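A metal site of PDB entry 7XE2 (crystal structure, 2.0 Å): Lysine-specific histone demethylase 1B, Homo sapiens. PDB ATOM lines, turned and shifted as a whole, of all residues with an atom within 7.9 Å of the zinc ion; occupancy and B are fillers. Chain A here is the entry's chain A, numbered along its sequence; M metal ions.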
ATOM      1  N   LYS A  23      -5.962  -8.566   7.214  1.00  0.00           N
ATOM      2  CA  LYS A  23      -6.609  -7.285   6.952  1.00  0.00           C
ATOM      3  C   LYS A  23      -5.863  -6.123   7.602  1.00  0.00           C
ATOM      4  O   LYS A  23      -5.044  -6.298   8.513  1.00  0.00           O
ATOM      5  CB  LYS A  23      -8.051  -7.292   7.463  1.00  0.00           C
ATOM      6  CG  LYS A  23      -8.970  -8.241   6.721  1.00  0.00           C
ATOM      7  CD  LYS A  23      -9.045  -7.852   5.252  1.00  0.00           C
ATOM      8  CE  LYS A  23     -10.076  -8.693   4.495  1.00  0.00           C
ATOM      9  NZ  LYS A  23     -10.168  -8.271   3.070  1.00  0.00           N
ATOM     10  N   CYS A  24      -6.180  -4.923   7.130  1.00  0.00           N
ATOM     11  CA  CYS A  24      -5.639  -3.703   7.700  1.00  0.00           C
ATOM     12  C   CYS A  24      -6.102  -3.528   9.145  1.00  0.00           C
ATOM     13  O   CYS A  24      -7.201  -3.933   9.527  1.00  0.00           O
ATOM     14  CB  CYS A  24      -6.065  -2.510   6.836  1.00  0.00           C
ATOM     15  SG  CYS A  24      -5.643  -0.925   7.513  1.00  0.00           S
ATOM     16  N   GLU A  25      -5.225  -2.933   9.960  1.00  0.00           N
ATOM     17  CA  GLU A  25      -5.565  -2.517  11.321  1.00  0.00           C
ATOM     18  C   GLU A  25      -6.767  -1.578  11.393  1.00  0.00           C
ATOM     19  O   GLU A  25      -7.383  -1.465  12.454  1.00  0.00           O
ATOM     20  CB  GLU A  25      -4.364  -1.793  11.953  1.00  0.00           C
ATOM     21  CG  GLU A  25      -4.129  -0.409  11.308  1.00  0.00           C
ATOM     22  CD  GLU A  25      -3.007   0.404  11.933  1.00  0.00           C
ATOM     23  OE1 GLU A  25      -2.658   0.148  13.105  1.00  0.00           O
ATOM     24  OE2 GLU A  25      -2.477   1.312  11.261  1.00  0.00           O
ATOM     25  N   LYS A  26      -7.107  -0.857  10.324  1.00  0.00           N
ATOM     26  CA  LYS A  26      -8.089   0.221  10.396  1.00  0.00           C
ATOM     27  C   LYS A  26      -9.460  -0.281   9.981  1.00  0.00           C
ATOM     28  O   LYS A  26      -9.654  -0.686   8.825  1.00  0.00           O
ATOM     29  CB  LYS A  26      -7.696   1.402   9.530  1.00  0.00           C
ATOM     30  CG  LYS A  26      -8.829   2.428   9.360  1.00  0.00           C
ATOM     31  CD  LYS A  26      -8.789   3.538  10.413  1.00  0.00           C
ATOM     32  CE  LYS A  26     -10.081   4.377  10.436  1.00  0.00           C
ATOM     33  NZ  LYS A  26     -11.175   3.750  11.246  1.00  0.00           N
ATOM     34  N   ALA A  27     -10.419  -0.216  10.903  1.00  0.00           N
ATOM     35  CA  ALA A  27     -11.818  -0.485  10.590  1.00  0.00           C
ATOM     36  C   ALA A  27     -12.280   0.362   9.409  1.00  0.00           C
ATOM     37  O   ALA A  27     -12.117   1.589   9.394  1.00  0.00           O
ATOM     38  CB  ALA A  27     -12.695  -0.191  11.812  1.00  0.00           C
ATOM     39  N   GLY A  28     -12.840  -0.307   8.402  1.00  0.00           N
ATOM     40  CA  GLY A  28     -13.401   0.412   7.276  1.00  0.00           C
ATOM     41  C   GLY A  28     -12.447   0.694   6.138  1.00  0.00           C
ATOM     42  O   GLY A  28     -12.873   1.269   5.129  1.00  0.00           O
ATOM     43  N   CYS A  29     -11.176   0.313   6.273  1.00  0.00           N
ATOM     44  CA  CYS A  29     -10.234   0.533   5.181  1.00  0.00           C
ATOM     45  C   CYS A  29     -10.664  -0.231   3.934  1.00  0.00           C
ATOM     46  O   CYS A  29     -11.122  -1.362   4.020  1.00  0.00           O
ATOM     47  CB  CYS A  29      -8.834   0.090   5.618  1.00  0.00           C
ATOM     48  SG  CYS A  29      -7.611   0.256   4.333  1.00  0.00           S
ATOM     49  N   THR A  30     -10.506   0.383   2.766  1.00  0.00           N
ATOM     50  CA  THR A  30     -11.018  -0.256   1.560  1.00  0.00           C
ATOM     51  C   THR A  30     -10.063  -1.272   0.941  1.00  0.00           C
ATOM     52  O   THR A  30     -10.473  -1.968   0.020  1.00  0.00           O
ATOM     53  CB  THR A  30     -11.351   0.794   0.496  1.00  0.00           C
ATOM     54  OG1 THR A  30     -10.178   1.570   0.261  1.00  0.00           O
ATOM     55  CG2 THR A  30     -12.463   1.692   0.972  1.00  0.00           C
ATOM     56  N   ALA A  31      -8.811  -1.345   1.387  1.00  0.00           N
ATOM     57  CA  ALA A  31      -7.878  -2.302   0.798  1.00  0.00           C
ATOM     58  C   ALA A  31      -8.249  -3.712   1.242  1.00  0.00           C
ATOM     59  O   ALA A  31      -8.054  -4.077   2.404  1.00  0.00           O
ATOM     60  CB  ALA A  31      -6.444  -1.961   1.213  1.00  0.00           C
ATOM     61  N   THR A  32      -8.790  -4.518   0.316  1.00  0.00           N
ATOM     62  CA  THR A  32      -9.106  -5.901   0.697  1.00  0.00           C
ATOM     63  C   THR A  32      -7.841  -6.715   0.911  1.00  0.00           C
ATOM     64  O   THR A  32      -7.823  -7.622   1.739  1.00  0.00           O
ATOM     65  CB  THR A  32      -9.994  -6.570  -0.359  1.00  0.00           C
ATOM     66  OG1 THR A  32      -9.485  -6.279  -1.663  1.00  0.00           O
ATOM     67  CG2 THR A  32     -11.414  -6.060  -0.242  1.00  0.00           C
ATOM     68  N   PRO A  34      -4.062  -5.753   1.747  1.00  0.00           N
ATOM     69  CA  PRO A  34      -2.918  -4.859   1.987  1.00  0.00           C
ATOM     70  C   PRO A  34      -1.634  -5.544   1.574  1.00  0.00           C
ATOM     71  O   PRO A  34      -1.449  -6.738   1.811  1.00  0.00           O
ATOM     72  CB  PRO A  34      -2.957  -4.612   3.493  1.00  0.00           C
ATOM     73  CG  PRO A  34      -4.306  -5.049   3.949  1.00  0.00           C
ATOM     74  CD  PRO A  34      -4.763  -6.097   2.997  1.00  0.00           C
ATOM     75  N   TRP A  53      -0.992  -4.861  10.184  1.00  0.00           N
ATOM     76  CA  TRP A  53      -0.850  -4.101   8.944  1.00  0.00           C
ATOM     77  C   TRP A  53      -1.034  -2.611   9.269  1.00  0.00           C
ATOM     78  O   TRP A  53      -2.141  -2.174   9.604  1.00  0.00           O
ATOM     79  CB  TRP A  53      -1.859  -4.563   7.892  1.00  0.00           C
ATOM     80  CG  TRP A  53      -1.409  -5.742   7.062  1.00  0.00           C
ATOM     81  CD1 TRP A  53      -1.929  -7.010   7.089  1.00  0.00           C
ATOM     82  CD2 TRP A  53      -0.354  -5.759   6.103  1.00  0.00           C
ATOM     83  NE1 TRP A  53      -1.241  -7.818   6.195  1.00  0.00           N
ATOM     84  CE2 TRP A  53      -0.272  -7.064   5.581  1.00  0.00           C
ATOM     85  CE3 TRP A  53       0.550  -4.797   5.637  1.00  0.00           C
ATOM     86  CZ2 TRP A  53       0.660  -7.435   4.606  1.00  0.00           C
ATOM     87  CZ3 TRP A  53       1.476  -5.153   4.669  1.00  0.00           C
ATOM     88  CH2 TRP A  53       1.527  -6.465   4.162  1.00  0.00           C
ATOM     89  N   TYR A  54       0.031  -1.832   9.177  1.00  0.00           N
ATOM     90  CA  TYR A  54      -0.035  -0.431   9.537  1.00  0.00           C
ATOM     91  C   TYR A  54      -0.580   0.382   8.373  1.00  0.00           C
ATOM     92  O   TYR A  54      -0.092   0.260   7.245  1.00  0.00           O
ATOM     93  CB  TYR A  54       1.358   0.070   9.956  1.00  0.00           C
ATOM     94  CG  TYR A  54       1.837  -0.535  11.267  1.00  0.00           C
ATOM     95  CD1 TYR A  54       2.456  -1.788  11.305  1.00  0.00           C
ATOM     96  CD2 TYR A  54       1.642   0.122  12.467  1.00  0.00           C
ATOM     97  CE1 TYR A  54       2.881  -2.339  12.495  1.00  0.00           C
ATOM     98  CE2 TYR A  54       2.048  -0.419  13.663  1.00  0.00           C
ATOM     99  CZ  TYR A  54       2.663  -1.647  13.676  1.00  0.00           C
ATOM    100  OH  TYR A  54       3.064  -2.173  14.879  1.00  0.00           O
ATOM    101  N   HIS A  55      -1.593   1.213   8.651  1.00  0.00           N
ATOM    102  CA  HIS A  55      -2.310   1.985   7.641  1.00  0.00           C
ATOM    103  C   HIS A  55      -1.767   3.401   7.531  1.00  0.00           C
ATOM    104  O   HIS A  55      -1.827   4.166   8.499  1.00  0.00           O
ATOM    105  CB  HIS A  55      -3.796   2.015   8.005  1.00  0.00           C
ATOM    106  CG  HIS A  55      -4.638   2.903   7.130  1.00  0.00           C
ATOM    107  ND1 HIS A  55      -5.511   2.398   6.183  1.00  0.00           N
ATOM    108  CD2 HIS A  55      -4.791   4.251   7.097  1.00  0.00           C
ATOM    109  CE1 HIS A  55      -6.149   3.388   5.596  1.00  0.00           C
ATOM    110  NE2 HIS A  55      -5.727   4.526   6.129  1.00  0.00           N
ATOM    111  N   LEU A  56      -1.272   3.768   6.348  1.00  0.00           N
ATOM    112  CA  LEU A  56      -1.019   5.153   5.985  1.00  0.00           C
ATOM    113  C   LEU A  56      -2.168   5.765   5.191  1.00  0.00           C
ATOM    114  O   LEU A  56      -2.579   6.890   5.469  1.00  0.00           O
ATOM    115  CB  LEU A  56       0.264   5.272   5.161  1.00  0.00           C
ATOM    116  CG  LEU A  56       1.580   5.082   5.911  1.00  0.00           C
ATOM    117  CD1 LEU A  56       2.729   5.346   4.970  1.00  0.00           C
ATOM    118  CD2 LEU A  56       1.641   6.008   7.112  1.00  0.00           C
ATOM    119  N   SER A  57      -2.695   5.020   4.210  1.00  0.00           N
ATOM    120  CA  SER A  57      -3.847   5.416   3.419  1.00  0.00           C
ATOM    121  C   SER A  57      -4.561   4.144   2.984  1.00  0.00           C
ATOM    122  O   SER A  57      -4.074   3.033   3.192  1.00  0.00           O
ATOM    123  CB  SER A  57      -3.443   6.248   2.184  1.00  0.00           C
ATOM    124  OG  SER A  57      -2.904   5.410   1.170  1.00  0.00           O
ATOM    125  N   CYS A  58      -5.721   4.315   2.361  1.00  0.00           N
ATOM    126  CA  CYS A  58      -6.442   3.150   1.829  1.00  0.00           C
ATOM    127  C   CYS A  58      -5.623   2.372   0.816  1.00  0.00           C
ATOM    128  O   CYS A  58      -5.889   1.192   0.618  1.00  0.00           O
ATOM    129  CB  CYS A  58      -7.777   3.580   1.212  1.00  0.00           C
ATOM    130  SG  CYS A  58      -9.003   3.989   2.481  1.00  0.00           S
ATOM    131  N   GLY A  59      -4.604   2.971   0.220  1.00  0.00           N
ATOM    132  CA  GLY A  59      -3.810   2.265  -0.766  1.00  0.00           C
ATOM    133  C   GLY A  59      -2.417   1.884  -0.307  1.00  0.00           C
ATOM    134  O   GLY A  59      -1.686   1.223  -1.055  1.00  0.00           O
ATOM    135  N   GLU A  60      -2.040   2.231   0.925  1.00  0.00           N
ATOM    136  CA  GLU A  60      -0.643   2.134   1.352  1.00  0.00           C
ATOM    137  C   GLU A  60      -0.549   1.584   2.761  1.00  0.00           C
ATOM    138  O   GLU A  60      -1.080   2.189   3.701  1.00  0.00           O
ATOM    139  CB  GLU A  60       0.041   3.505   1.235  1.00  0.00           C
ATOM    140  CG  GLU A  60       0.141   3.957  -0.225  1.00  0.00           C
ATOM    141  CD  GLU A  60       0.224   5.447  -0.399  1.00  0.00           C
ATOM    142  OE1 GLU A  60      -0.591   6.178   0.199  1.00  0.00           O
ATOM    143  OE2 GLU A  60       1.112   5.892  -1.179  1.00  0.00           O
ATOM    144  N   HIS A  61       0.160   0.464   2.915  1.00  0.00           N
ATOM    145  CA  HIS A  61       0.297  -0.225   4.185  1.00  0.00           C
ATOM    146  C   HIS A  61       1.714  -0.756   4.296  1.00  0.00           C
ATOM    147  O   HIS A  61       2.402  -0.945   3.290  1.00  0.00           O
ATOM    148  CB  HIS A  61      -0.741  -1.374   4.326  1.00  0.00           C
ATOM    149  CG  HIS A  61      -2.158  -0.922   4.141  1.00  0.00           C
ATOM    150  ND1 HIS A  61      -2.724  -0.750   2.902  1.00  0.00           N
ATOM    151  CD2 HIS A  61      -3.116  -0.571   5.041  1.00  0.00           C
ATOM    152  CE1 HIS A  61      -3.963  -0.308   3.034  1.00  0.00           C
ATOM    153  NE2 HIS A  61      -4.227  -0.187   4.332  1.00  0.00           N
ATOM    154  N   MET A 175      -9.490   9.059   5.139  1.00  0.00           N
ATOM    155  CA  MET A 175      -8.791   7.875   5.627  1.00  0.00           C
ATOM    156  C   MET A 175      -7.279   8.013   5.599  1.00  0.00           C
ATOM    157  O   MET A 175      -6.569   7.040   5.921  1.00  0.00           O
ATOM    158  CB  MET A 175      -9.169   6.644   4.784  1.00  0.00           C
ATOM    159  CG  MET A 175     -10.655   6.435   4.702  1.00  0.00           C
ATOM    160  SD  MET A 175     -11.285   5.821   6.255  1.00  0.00           S
ATOM    161  CE  MET A 175     -10.654   4.137   6.139  1.00  0.00           C
HETATM  162 ZN    ZN M   1      -5.709   0.367   5.583  1.00  0.00          ZN
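SG of Cys 24 lies close to N of Lys 26, 3.2 Å away.
SG of Cys 29 sits close to N of Ala 31, 3.6 Å away.
The side-chain hydroxyl (OG) of Ser 57 sits at hydrogen-bond distance from the side-chain carboxylate (OE1) of Glu 60, 2.6 Å away.
The backbone carbonyl oxygen of Ser 57 lies close to a ring nitrogen (ND1) of His 55, 3.4 Å away.
A ring nitrogen (NE2) of His 55 is in hydrogen-bond range of the backbone carbonyl oxygen of Met 175, 2.7 Å away.
N of Gly 59 lies close to OG of Ser 57 (3.1 Å).
The backbone NH (N) of His 55 is in hydrogen-bond range of the side-chain carboxylate (OE2) of Glu 25.
The backbone carbonyl oxygen of Ser 57 lies close to a ring nitrogen (NE2) of His 61.
Residues that only touch the zinc ion: Ser 57 (3.9 Å).
Within 4 Å of the zinc ion: Cys 24, Cys 29, His 55, Ser 57 and His 61.
NE2 of His 61 is bound to the zinc ion (2.0 Å).
The zinc ion is bound by ND1 of His 55 (2.1 Å).
The zinc ion is bound by SG of Cys 29, at 2.3 Å.
SG of Cys 24 is bound to the zinc ion (2.3 Å).
The zinc ion has four donor atoms within binding distance.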
